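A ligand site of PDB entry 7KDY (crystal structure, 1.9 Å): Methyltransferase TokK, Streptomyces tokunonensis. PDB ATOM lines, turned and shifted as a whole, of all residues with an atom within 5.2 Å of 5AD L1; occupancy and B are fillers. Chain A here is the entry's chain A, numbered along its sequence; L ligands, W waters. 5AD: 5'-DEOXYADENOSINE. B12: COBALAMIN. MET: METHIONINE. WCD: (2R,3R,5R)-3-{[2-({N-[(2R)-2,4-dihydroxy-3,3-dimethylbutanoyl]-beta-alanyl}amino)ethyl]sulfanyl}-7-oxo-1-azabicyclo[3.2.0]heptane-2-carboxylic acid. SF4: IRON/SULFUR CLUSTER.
N6 of 5AD L1 lies within hydrogen-bond range of O of Phe 212, 3.0 Å away.
The backbone carbonyl oxygen (O) of Gly 384 lies within hydrogen-bond range of a nitrogen (N6) of 5AD L1 (3.0 Å).
An oxygen (O28) of B12 L2 lies within hydrogen-bond range of the backbone NH (N) of Trp 215 (3.1 Å).
An oxygen (O08) of WCD L4 sits at hydrogen-bond distance from the side-chain amide nitrogen (ND2) of Asn 282, 3.1 Å away.
The side-chain carboxylate (OE1) of Glu 349 sits at hydrogen-bond distance from an oxygen (O3') of 5AD L1 (2.6 Å).
An oxygen (O2') of 5AD L1 sits at hydrogen-bond distance from the side-chain amide oxygen of Gln 312 (2.7 Å).
N of Gly 384 is in hydrogen-bond range of N1 of 5AD L1, 3.1 Å away.
An iron atom (FE4) of SF4 L5 is bound by the side-chain sulfur of Cys 213 (2.5 Å).
OG of Ser 310 lies within hydrogen-bond range of OE1 of Glu 349, 2.5 Å away.
OE2 of Glu 349 is in hydrogen-bond range of OH of Tyr 381 (2.6 Å).
The backbone carbonyl oxygen (O) of Leu 350 is in hydrogen-bond range of the backbone NH (N) of Tyr 381 (3.1 Å).
N of Ile 351 sits at hydrogen-bond distance from O of Gln 312 (3.0 Å).
N of Trp 215 sits close to SG of Cys 213, at 3.4 Å.
The backbone NH (N) of Gln 312 lies within hydrogen-bond range of the backbone carbonyl oxygen (O) of Glu 349 (2.9 Å).
N29 of B12 L2 lies within hydrogen-bond range of N7 of 5AD L1.
O3' of 5AD L1 lies close to SD of MET L3 (3.5 Å).
FE3 of SF4 L5 is bound by O of MET L3.
Water W1 lies within hydrogen-bond range of a nitrogen (N40) of B12 L2 (2.7 Å) and an oxygen (O4') of 5AD L1 (2.9 Å).
Merely in contact with 5AD L1: Glu 382 (3.4 Å), Tyr 381 (3.4 Å), Asn 282 (3.5 Å), Trp 215 (3.5 Å), Ile 351 (3.7 Å), Leu 386 (3.8 Å) and Leu 383 (3.9 Å).
Hydrophobic or aromatic side chains within 4 Å of 5AD L1: Phe 212, Trp 215, Ile 351, Tyr 381, Leu 383 and Leu 386.
11 residues have an atom within 4 Å of 5AD L1: Phe 212, Trp 215, Asn 282, Gln 312, Glu 349, Ile 351, Tyr 381, Glu 382, Leu 383, Gly 384 and Leu 386.
The nearest printed residue that does not touch 5AD L1 is Ser 310 (4.1 Å).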
ATOM      1  N   PHE A 212      19.161   5.836  -4.499  1.00  0.00           N
ATOM      2  CA  PHE A 212      18.024   5.662  -5.393  1.00  0.00           C
ATOM      3  C   PHE A 212      18.080   6.553  -6.625  1.00  0.00           C
ATOM      4  O   PHE A 212      17.330   6.304  -7.578  1.00  0.00           O
ATOM      5  CB  PHE A 212      16.714   5.938  -4.641  1.00  0.00           C
ATOM      6  CG  PHE A 212      16.638   7.328  -4.049  1.00  0.00           C
ATOM      7  CD1 PHE A 212      16.358   8.431  -4.846  1.00  0.00           C
ATOM      8  CD2 PHE A 212      16.856   7.523  -2.690  1.00  0.00           C
ATOM      9  CE1 PHE A 212      16.312   9.709  -4.306  1.00  0.00           C
ATOM     10  CE2 PHE A 212      16.797   8.796  -2.147  1.00  0.00           C
ATOM     11  CZ  PHE A 212      16.520   9.884  -2.950  1.00  0.00           C
ATOM     12  N   CYS A 213      18.943   7.558  -6.641  1.00  0.00           N
ATOM     13  CA  CYS A 213      18.876   8.648  -7.602  1.00  0.00           C
ATOM     14  C   CYS A 213      19.869   8.467  -8.745  1.00  0.00           C
ATOM     15  O   CYS A 213      20.917   7.850  -8.598  1.00  0.00           O
ATOM     16  CB  CYS A 213      19.140   9.986  -6.901  1.00  0.00           C
ATOM     17  SG  CYS A 213      18.790  11.417  -7.917  1.00  0.00           S
ATOM     18  N   TRP A 215      20.279  11.491 -10.945  1.00  0.00           N
ATOM     19  CA  TRP A 215      20.031  12.838 -11.447  1.00  0.00           C
ATOM     20  C   TRP A 215      21.041  13.238 -12.523  1.00  0.00           C
ATOM     21  O   TRP A 215      22.242  13.354 -12.248  1.00  0.00           O
ATOM     22  CB  TRP A 215      20.086  13.836 -10.292  1.00  0.00           C
ATOM     23  CG  TRP A 215      19.333  15.092 -10.579  1.00  0.00           C
ATOM     24  CD1 TRP A 215      19.829  16.278 -11.035  1.00  0.00           C
ATOM     25  CD2 TRP A 215      17.911  15.280 -10.452  1.00  0.00           C
ATOM     26  NE1 TRP A 215      18.827  17.198 -11.180  1.00  0.00           N
ATOM     27  CE2 TRP A 215      17.631  16.613 -10.832  1.00  0.00           C
ATOM     28  CE3 TRP A 215      16.864  14.453 -10.052  1.00  0.00           C
ATOM     29  CZ2 TRP A 215      16.336  17.127 -10.827  1.00  0.00           C
ATOM     30  CZ3 TRP A 215      15.576  14.964 -10.055  1.00  0.00           C
ATOM     31  CH2 TRP A 215      15.329  16.292 -10.431  1.00  0.00           C
ATOM     32  N   ASN A 282      14.417  22.264  -8.559  1.00  0.00           N
ATOM     33  CA  ASN A 282      14.702  21.589  -7.311  1.00  0.00           C
ATOM     34  C   ASN A 282      15.758  22.382  -6.547  1.00  0.00           C
ATOM     35  O   ASN A 282      16.851  22.625  -7.066  1.00  0.00           O
ATOM     36  CB  ASN A 282      15.190  20.166  -7.569  1.00  0.00           C
ATOM     37  CG  ASN A 282      14.059  19.244  -7.981  1.00  0.00           C
ATOM     38  OD1 ASN A 282      13.384  18.670  -7.126  1.00  0.00           O
ATOM     39  ND2 ASN A 282      13.846  19.104  -9.282  1.00  0.00           N
ATOM     40  N   SER A 310      13.305  18.653   0.851  1.00  0.00           N
ATOM     41  CA  SER A 310      12.931  17.251   0.761  1.00  0.00           C
ATOM     42  C   SER A 310      13.763  16.381   1.691  1.00  0.00           C
ATOM     43  O   SER A 310      14.880  16.725   2.076  1.00  0.00           O
ATOM     44  CB  SER A 310      13.040  16.753  -0.675  1.00  0.00           C
ATOM     45  OG  SER A 310      11.951  17.216  -1.464  1.00  0.00           O
ATOM     46  N   GLN A 312      13.061  12.490   1.677  1.00  0.00           N
ATOM     47  CA  GLN A 312      12.951  11.111   1.205  1.00  0.00           C
ATOM     48  C   GLN A 312      12.536  10.184   2.349  1.00  0.00           C
ATOM     49  O   GLN A 312      11.579   9.418   2.227  1.00  0.00           O
ATOM     50  CB  GLN A 312      14.259  10.628   0.556  1.00  0.00           C
ATOM     51  CG  GLN A 312      15.034  11.701  -0.222  1.00  0.00           C
ATOM     52  CD  GLN A 312      14.227  12.370  -1.331  1.00  0.00           C
ATOM     53  OE1 GLN A 312      13.083  11.998  -1.601  1.00  0.00           O
ATOM     54  NE2 GLN A 312      14.847  13.333  -1.998  1.00  0.00           N
ATOM     55  N   GLU A 349       9.404  16.177  -0.109  1.00  0.00           N
ATOM     56  CA  GLU A 349       9.152  14.911  -0.791  1.00  0.00           C
ATOM     57  C   GLU A 349       9.613  13.733   0.068  1.00  0.00           C
ATOM     58  O   GLU A 349      10.620  13.815   0.772  1.00  0.00           O
ATOM     59  CB  GLU A 349       9.870  14.855  -2.139  1.00  0.00           C
ATOM     60  CG  GLU A 349       9.365  15.893  -3.132  1.00  0.00           C
ATOM     61  CD  GLU A 349      10.389  16.191  -4.196  1.00  0.00           C
ATOM     62  OE1 GLU A 349      11.580  16.380  -3.843  1.00  0.00           O
ATOM     63  OE2 GLU A 349      10.007  16.239  -5.381  1.00  0.00           O
ATOM     64  N   LEU A 350       8.842  12.654   0.020  1.00  0.00           N
ATOM     65  CA  LEU A 350       9.208  11.378   0.614  1.00  0.00           C
ATOM     66  C   LEU A 350       9.099  10.297  -0.447  1.00  0.00           C
ATOM     67  O   LEU A 350       8.353  10.429  -1.424  1.00  0.00           O
ATOM     68  CB  LEU A 350       8.285  11.021   1.803  1.00  0.00           C
ATOM     69  CG  LEU A 350       8.255  11.968   3.006  1.00  0.00           C
ATOM     70  CD1 LEU A 350       7.143  11.563   3.960  1.00  0.00           C
ATOM     71  CD2 LEU A 350       9.600  11.968   3.719  1.00  0.00           C
ATOM     72  N   ILE A 351       9.859   9.221  -0.250  1.00  0.00           N
ATOM     73  CA  ILE A 351       9.805   8.057  -1.126  1.00  0.00           C
ATOM     74  C   ILE A 351       9.323   6.878  -0.303  1.00  0.00           C
ATOM     75  O   ILE A 351       9.854   6.603   0.783  1.00  0.00           O
ATOM     76  CB  ILE A 351      11.176   7.757  -1.768  1.00  0.00           C
ATOM     77  CG1 ILE A 351      11.642   8.937  -2.616  1.00  0.00           C
ATOM     78  CG2 ILE A 351      11.081   6.488  -2.611  1.00  0.00           C
ATOM     79  CD1 ILE A 351      13.006   8.727  -3.235  1.00  0.00           C
ATOM     80  N   TYR A 381       6.439   9.617  -3.669  1.00  0.00           N
ATOM     81  CA  TYR A 381       6.651   8.863  -4.903  1.00  0.00           C
ATOM     82  C   TYR A 381       6.906   7.407  -4.566  1.00  0.00           C
ATOM     83  O   TYR A 381       7.581   7.102  -3.577  1.00  0.00           O
ATOM     84  CB  TYR A 381       7.852   9.408  -5.699  1.00  0.00           C
ATOM     85  CG  TYR A 381       7.854  10.906  -5.861  1.00  0.00           C
ATOM     86  CD1 TYR A 381       6.938  11.542  -6.683  1.00  0.00           C
ATOM     87  CD2 TYR A 381       8.785  11.682  -5.182  1.00  0.00           C
ATOM     88  CE1 TYR A 381       6.943  12.911  -6.823  1.00  0.00           C
ATOM     89  CE2 TYR A 381       8.797  13.057  -5.318  1.00  0.00           C
ATOM     90  CZ  TYR A 381       7.875  13.665  -6.138  1.00  0.00           C
ATOM     91  OH  TYR A 381       7.880  15.034  -6.278  1.00  0.00           O
ATOM     92  N   GLU A 382       6.358   6.500  -5.385  1.00  0.00           N
ATOM     93  CA  GLU A 382       6.756   5.108  -5.315  1.00  0.00           C
ATOM     94  C   GLU A 382       8.221   4.975  -5.724  1.00  0.00           C
ATOM     95  O   GLU A 382       8.645   5.558  -6.722  1.00  0.00           O
ATOM     96  CB  GLU A 382       5.913   4.237  -6.241  1.00  0.00           C
ATOM     97  CG  GLU A 382       4.410   4.385  -6.091  1.00  0.00           C
ATOM     98  CD  GLU A 382       3.829   5.302  -7.143  1.00  0.00           C
ATOM     99  OE1 GLU A 382       4.379   6.414  -7.324  1.00  0.00           O
ATOM    100  OE2 GLU A 382       2.829   4.920  -7.792  1.00  0.00           O
ATOM    101  N   LEU A 383       8.985   4.191  -4.965  1.00  0.00           N
ATOM    102  CA  LEU A 383      10.382   3.993  -5.282  1.00  0.00           C
ATOM    103  C   LEU A 383      10.541   3.234  -6.597  1.00  0.00           C
ATOM    104  O   LEU A 383       9.983   2.152  -6.773  1.00  0.00           O
ATOM    105  CB  LEU A 383      11.086   3.230  -4.154  1.00  0.00           C
ATOM    106  CG  LEU A 383      12.533   2.814  -4.442  1.00  0.00           C
ATOM    107  CD1 LEU A 383      13.403   4.034  -4.729  1.00  0.00           C
ATOM    108  CD2 LEU A 383      13.100   2.032  -3.277  1.00  0.00           C
ATOM    109  N   GLY A 384      11.294   3.815  -7.521  1.00  0.00           N
ATOM    110  CA  GLY A 384      11.655   3.160  -8.762  1.00  0.00           C
ATOM    111  C   GLY A 384      13.116   2.753  -8.737  1.00  0.00           C
ATOM    112  O   GLY A 384      13.961   3.475  -8.207  1.00  0.00           O
ATOM    113  N   ILE A 385      13.397   1.577  -9.306  1.00  0.00           N
ATOM    114  CA  ILE A 385      14.763   1.127  -9.506  1.00  0.00           C
ATOM    115  C   ILE A 385      15.198   1.647 -10.875  1.00  0.00           C
ATOM    116  O   ILE A 385      14.765   1.140 -11.910  1.00  0.00           O
ATOM    117  CB  ILE A 385      14.887  -0.396  -9.419  1.00  0.00           C
ATOM    118  CG1 ILE A 385      14.319  -0.884  -8.076  1.00  0.00           C
ATOM    119  CG2 ILE A 385      16.336  -0.823  -9.570  1.00  0.00           C
ATOM    120  CD1 ILE A 385      14.998  -0.303  -6.870  1.00  0.00           C
ATOM    121  N   LEU A 386      16.030   2.689 -10.872  1.00  0.00           N
ATOM    122  CA  LEU A 386      16.480   3.252 -12.133  1.00  0.00           C
ATOM    123  C   LEU A 386      17.673   2.446 -12.664  1.00  0.00           C
ATOM    124  O   LEU A 386      18.511   1.998 -11.875  1.00  0.00           O
ATOM    125  CB  LEU A 386      16.888   4.719 -11.953  1.00  0.00           C
ATOM    126  CG  LEU A 386      15.800   5.592 -11.326  1.00  0.00           C
ATOM    127  CD1 LEU A 386      16.287   7.023 -11.124  1.00  0.00           C
ATOM    128  CD2 LEU A 386      14.528   5.544 -12.164  1.00  0.00           C
ATOM    129  N   PHE A 424       7.934   0.939 -15.431  1.00  0.00           N
ATOM    130  CA  PHE A 424       8.668   1.592 -14.355  1.00  0.00           C
ATOM    131  C   PHE A 424       8.914   0.533 -13.294  1.00  0.00           C
ATOM    132  O   PHE A 424       7.958  -0.016 -12.730  1.00  0.00           O
ATOM    133  CB  PHE A 424       7.825   2.749 -13.809  1.00  0.00           C
ATOM    134  CG  PHE A 424       8.452   3.515 -12.679  1.00  0.00           C
ATOM    135  CD1 PHE A 424       9.337   4.553 -12.935  1.00  0.00           C
ATOM    136  CD2 PHE A 424       8.108   3.253 -11.366  1.00  0.00           C
ATOM    137  CE1 PHE A 424       9.889   5.282 -11.897  1.00  0.00           C
ATOM    138  CE2 PHE A 424       8.647   3.979 -10.325  1.00  0.00           C
ATOM    139  CZ  PHE A 424       9.548   5.006 -10.591  1.00  0.00           C
HETATM  140  N1  5AD L   1      12.118   6.835  -7.255  1.00  0.00           N
HETATM  141  C2  5AD L   1      11.209   7.720  -6.826  1.00  0.00           C
HETATM  142  N3  5AD L   1      11.362   9.026  -6.591  1.00  0.00           N
HETATM  143  C4  5AD L   1      12.606   9.433  -6.868  1.00  0.00           C
HETATM  144  N9  5AD L   1      13.126  10.694  -6.729  1.00  0.00           N
HETATM  145  C8  5AD L   1      14.422  10.609  -7.131  1.00  0.00           C
HETATM  146  N7  5AD L   1      14.795   9.396  -7.497  1.00  0.00           N
HETATM  147  C5  5AD L   1      13.636   8.644  -7.327  1.00  0.00           C
HETATM  148  C6  5AD L   1      13.371   7.270  -7.518  1.00  0.00           C
HETATM  149  N6  5AD L   1      14.309   6.405  -7.901  1.00  0.00           N
HETATM  150  C1' 5AD L   1      12.428  11.863  -6.198  1.00  0.00           C
HETATM  151  C2' 5AD L   1      12.984  12.364  -4.861  1.00  0.00           C
HETATM  152  C3' 5AD L   1      13.616  13.710  -5.245  1.00  0.00           C
HETATM  153  C4' 5AD L   1      12.741  14.149  -6.407  1.00  0.00           C
HETATM  154  C5' 5AD L   1      13.344  15.180  -7.329  1.00  0.00           C
HETATM  155  O4' 5AD L   1      12.525  12.922  -7.135  1.00  0.00           O
HETATM  156  O2' 5AD L   1      11.893  12.530  -3.955  1.00  0.00           O
HETATM  157  O3' 5AD L   1      13.545  14.674  -4.198  1.00  0.00           O
HETATM  158 CO   B12 L   2      12.133  13.221 -14.356  1.00  0.00          CO
HETATM  159  N21 B12 L   2      13.503  11.976 -14.024  1.00  0.00           N
HETATM  160  N22 B12 L   2      10.827  11.941 -13.766  1.00  0.00           N
HETATM  161  N23 B12 L   2      10.924  14.343 -15.343  1.00  0.00           N
HETATM  162  N24 B12 L   2      13.568  14.401 -14.709  1.00  0.00           N
HETATM  163  C1  B12 L   2      14.813  12.418 -14.494  1.00  0.00           C
HETATM  164  C20 B12 L   2      14.886  12.312 -16.004  1.00  0.00           C
HETATM  165  C2  B12 L   2      15.774  11.446 -13.696  1.00  0.00           C
HETATM  166  C25 B12 L   2      17.139  11.204 -14.345  1.00  0.00           C
HETATM  167  C26 B12 L   2      15.931  11.978 -12.261  1.00  0.00           C
HETATM  168  C27 B12 L   2      16.348  10.950 -11.186  1.00  0.00           C
HETATM  169  O28 B12 L   2      17.404  10.345 -11.298  1.00  0.00           O
HETATM  170  N29 B12 L   2      15.516  10.777 -10.164  1.00  0.00           N
HETATM  171  C3  B12 L   2      14.871  10.161 -13.578  1.00  0.00           C
HETATM  172  C30 B12 L   2      14.796   9.260 -14.826  1.00  0.00           C
HETATM  173  C31 B12 L   2      15.741   8.064 -14.831  1.00  0.00           C
HETATM  174  C32 B12 L   2      15.517   7.222 -16.072  1.00  0.00           C
HETATM  175  O34 B12 L   2      14.701   7.566 -16.935  1.00  0.00           O
HETATM  176  N33 B12 L   2      16.241   6.128 -16.164  1.00  0.00           N
HETATM  177  C4  B12 L   2      13.503  10.789 -13.503  1.00  0.00           C
HETATM  178  C5  B12 L   2      12.283  10.185 -12.932  1.00  0.00           C
HETATM  179  C35 B12 L   2      12.608   8.924 -12.190  1.00  0.00           C
HETATM  180  C6  B12 L   2      11.022  10.701 -13.163  1.00  0.00           C
HETATM  181  C7  B12 L   2       9.666  10.075 -12.831  1.00  0.00           C
HETATM  182  C36 B12 L   2       9.453   8.919 -13.826  1.00  0.00           C
HETATM  183  C37 B12 L   2       9.556   9.533 -11.374  1.00  0.00           C
HETATM  184  C38 B12 L   2       9.728  10.530 -10.214  1.00  0.00           C
HETATM  185  O39 B12 L   2       9.255  10.226  -9.116  1.00  0.00           O
HETATM  186  N40 B12 L   2      10.376  11.671 -10.428  1.00  0.00           N
HETATM  187  C8  B12 L   2       8.660  11.242 -13.054  1.00  0.00           C
HETATM  188  C41 B12 L   2       7.333  10.886 -13.742  1.00  0.00           C
HETATM  189  C42 B12 L   2       6.354  10.131 -12.843  1.00  0.00           C
HETATM  190  C43 B12 L   2       4.911  10.255 -13.258  1.00  0.00           C
HETATM  191  O44 B12 L   2       4.012  10.319 -12.417  1.00  0.00           O
HETATM  192  N45 B12 L   2       4.675  10.301 -14.559  1.00  0.00           N
HETATM  193  C9  B12 L   2       9.510  12.215 -13.825  1.00  0.00           C
HETATM  194  C10 B12 L   2       8.936  13.294 -14.489  1.00  0.00           C
HETATM  195  C11 B12 L   2       9.584  14.282 -15.218  1.00  0.00           C
HETATM  196  C12 B12 L   2       8.882  15.421 -15.910  1.00  0.00           C
HETATM  197  C46 B12 L   2       8.561  16.521 -14.879  1.00  0.00           C
HETATM  198  C47 B12 L   2       7.589  15.031 -16.654  1.00  0.00           C
HETATM  199  C13 B12 L   2      10.008  15.987 -16.813  1.00  0.00           C
HETATM  200  C48 B12 L   2      10.097  15.344 -18.215  1.00  0.00           C
HETATM  201  C49 B12 L   2      11.172  15.957 -19.106  1.00  0.00           C
HETATM  202  C50 B12 L   2      11.231  15.456 -20.528  1.00  0.00           C
HETATM  203  O51 B12 L   2      12.293  15.450 -21.157  1.00  0.00           O
HETATM  204  N52 B12 L   2      10.086  15.027 -21.035  1.00  0.00           N
HETATM  205  C14 B12 L   2      11.243  15.545 -16.027  1.00  0.00           C
HETATM  206  C15 B12 L   2      12.428  16.208 -15.903  1.00  0.00           C
HETATM  207  C53 B12 L   2      12.536  17.583 -16.501  1.00  0.00           C
HETATM  208  C16 B12 L   2      13.677  15.585 -15.259  1.00  0.00           C
HETATM  209  C17 B12 L   2      15.089  16.144 -15.132  1.00  0.00           C
HETATM  210  C54 B12 L   2      15.101  17.159 -13.978  1.00  0.00           C
HETATM  211  C55 B12 L   2      15.695  16.842 -16.391  1.00  0.00           C
HETATM  212  C56 B12 L   2      15.770  16.003 -17.664  1.00  0.00           C
HETATM  213  C57 B12 L   2      16.522  16.800 -18.695  1.00  0.00           C
HETATM  214  O58 B12 L   2      15.978  17.229 -19.700  1.00  0.00           O
HETATM  215  N59 B12 L   2      17.811  17.025 -18.441  1.00  0.00           N
HETATM  216  C18 B12 L   2      15.877  14.861 -14.835  1.00  0.00           C
HETATM  217  C60 B12 L   2      17.166  15.026 -14.012  1.00  0.00           C
HETATM  218  C61 B12 L   2      18.269  15.670 -14.821  1.00  0.00           C
HETATM  219  O63 B12 L   2      18.650  15.170 -15.887  1.00  0.00           O
HETATM  220  N62 B12 L   2      18.790  16.793 -14.343  1.00  0.00           N
HETATM  221  C19 B12 L   2      14.849  13.939 -14.145  1.00  0.00           C
HETATM  222  C1P B12 L   2      18.671  17.830 -19.293  1.00  0.00           C
HETATM  223  C2P B12 L   2      19.301  16.963 -20.431  1.00  0.00           C
HETATM  224  C3P B12 L   2      20.062  17.844 -21.384  1.00  0.00           C
HETATM  225  O3  B12 L   2      20.217  16.129 -19.824  1.00  0.00           O
HETATM  226  O4  B12 L   2      18.850  13.928 -19.648  1.00  0.00           O
HETATM  227  O5  B12 L   2      21.218  14.097 -18.795  1.00  0.00           O
HETATM  228  P   B12 L   2      20.189  14.541 -19.832  1.00  0.00           P
HETATM  229  O2  B12 L   2      20.807  14.298 -21.322  1.00  0.00           O
HETATM  230  C3R B12 L   2      22.190  14.074 -21.551  1.00  0.00           C
HETATM  231  C2R B12 L   2      22.603  12.593 -21.566  1.00  0.00           C
HETATM  232  O7R B12 L   2      21.568  11.767 -21.038  1.00  0.00           O
HETATM  233  C1R B12 L   2      22.848  12.344 -23.070  1.00  0.00           C
HETATM  234  O6R B12 L   2      23.281  13.565 -23.600  1.00  0.00           O
HETATM  235  C4R B12 L   2      22.566  14.619 -22.935  1.00  0.00           C
HETATM  236  C5R B12 L   2      23.389  15.886 -22.943  1.00  0.00           C
HETATM  237  O8R B12 L   2      24.668  15.674 -22.337  1.00  0.00           O
HETATM  238  N1B B12 L   2      21.704  11.857 -23.838  1.00  0.00           N
HETATM  239  C8B B12 L   2      21.841  11.387 -25.139  1.00  0.00           C
HETATM  240  C2B B12 L   2      20.361  12.036 -23.630  1.00  0.00           C
HETATM  241  N3B B12 L   2      19.621  11.713 -24.661  1.00  0.00           N
HETATM  242  C9B B12 L   2      20.534  11.296 -25.626  1.00  0.00           C
HETATM  243  C4B B12 L   2      20.339  10.849 -26.928  1.00  0.00           C
HETATM  244  C5B B12 L   2      21.421  10.499 -27.731  1.00  0.00           C
HETATM  245  C5M B12 L   2      21.177  10.002 -29.127  1.00  0.00           C
HETATM  246  C6B B12 L   2      22.735  10.611 -27.217  1.00  0.00           C
HETATM  247  C6M B12 L   2      23.931  10.305 -28.081  1.00  0.00           C
HETATM  248  C7B B12 L   2      22.934  11.051 -25.909  1.00  0.00           C
HETATM  249  N   MET L   3      18.859  17.681  -4.372  1.00  0.00           N
HETATM  250  CA  MET L   3      17.750  18.128  -3.524  1.00  0.00           C
HETATM  251  C   MET L   3      17.435  17.111  -2.434  1.00  0.00           C
HETATM  252  O   MET L   3      17.652  15.905  -2.573  1.00  0.00           O
HETATM  253  CB  MET L   3      16.507  18.407  -4.368  1.00  0.00           C
HETATM  254  CG  MET L   3      15.634  17.197  -4.665  1.00  0.00           C
HETATM  255  SD  MET L   3      16.416  15.966  -5.719  1.00  0.00           S
HETATM  256  CE  MET L   3      16.762  16.931  -7.180  1.00  0.00           C
HETATM  257  OXT MET L   3      16.939  17.475  -1.363  1.00  0.00           O
HETATM  258  C13 WCD L   4       0.192  11.827 -19.123  1.00  0.00           C
HETATM  259  C14 WCD L   4      -0.272  12.567 -16.788  1.00  0.00           C
HETATM  260  C15 WCD L   4      -1.669  13.419 -18.667  1.00  0.00           C
HETATM  261  C16 WCD L   4      -0.259  13.005 -18.246  1.00  0.00           C
HETATM  262  C18 WCD L   4       0.703  14.201 -18.425  1.00  0.00           C
HETATM  263  C19 WCD L   4       2.046  13.940 -17.728  1.00  0.00           C
HETATM  264  C21 WCD L   4       3.596  14.739 -15.978  1.00  0.00           C
HETATM  265  C22 WCD L   4       3.189  14.252 -14.581  1.00  0.00           C
HETATM  266  C23 WCD L   4       4.415  13.919 -13.725  1.00  0.00           C
HETATM  267  C01 WCD L   4       9.981  15.736  -8.735  1.00  0.00           C
HETATM  268  C02 WCD L   4      10.404  16.731  -9.823  1.00  0.00           C
HETATM  269  C04 WCD L   4       8.566  15.692  -9.362  1.00  0.00           C
HETATM  270  C05 WCD L   4       8.345  17.010 -11.418  1.00  0.00           C
HETATM  271  C06 WCD L   4       7.453  15.737 -11.386  1.00  0.00           C
HETATM  272  C07 WCD L   4       8.345  14.767 -10.553  1.00  0.00           C
HETATM  273  C09 WCD L   4       7.535  18.322 -11.424  1.00  0.00           C
HETATM  274  C24 WCD L   4       5.217  14.401 -10.242  1.00  0.00           C
HETATM  275  C26 WCD L   4       5.256  13.492 -11.473  1.00  0.00           C
HETATM  276  N03 WCD L   4       9.084  16.701 -10.230  1.00  0.00           N
HETATM  277  N20 WCD L   4       2.362  14.839 -16.782  1.00  0.00           N
HETATM  278  N27 WCD L   4       4.182  13.839 -12.406  1.00  0.00           N
HETATM  279  O08 WCD L   4      11.420  17.339 -10.154  1.00  0.00           O
HETATM  280  O10 WCD L   4       5.516  13.741 -14.251  1.00  0.00           O
HETATM  281  O11 WCD L   4       2.772  12.994 -18.029  1.00  0.00           O
HETATM  282  O12 WCD L   4      -0.718  10.746 -19.009  1.00  0.00           O
HETATM  283  O17 WCD L   4       0.105  15.361 -17.849  1.00  0.00           O
HETATM  284  O28 WCD L   4       7.173  18.786 -10.308  1.00  0.00           O
HETATM  285  O29 WCD L   4       7.328  18.856 -12.533  1.00  0.00           O
HETATM  286  S25 WCD L   4       5.867  16.088 -10.563  1.00  0.00           S
HETATM  287 FE1  SF4 L   5      20.192  13.104  -3.567  1.00  0.00          FE
HETATM  288 FE2  SF4 L   5      21.415  14.669  -5.340  1.00  0.00          FE
HETATM  289 FE3  SF4 L   5      18.824  15.253  -4.586  1.00  0.00          FE
HETATM  290 FE4  SF4 L   5      19.430  13.053  -6.136  1.00  0.00          FE
HETATM  291  S1  SF4 L   5      19.703  15.201  -6.712  1.00  0.00           S
HETATM  292  S2  SF4 L   5      18.051  13.114  -4.331  1.00  0.00           S
HETATM  293  S3  SF4 L   5      21.443  12.437  -5.313  1.00  0.00           S
HETATM  294  S4  SF4 L   5      20.722  15.238  -3.255  1.00  0.00           S
HETATM  295  O   HOH W   1      13.004  12.266  -9.902  1.00  0.00           O
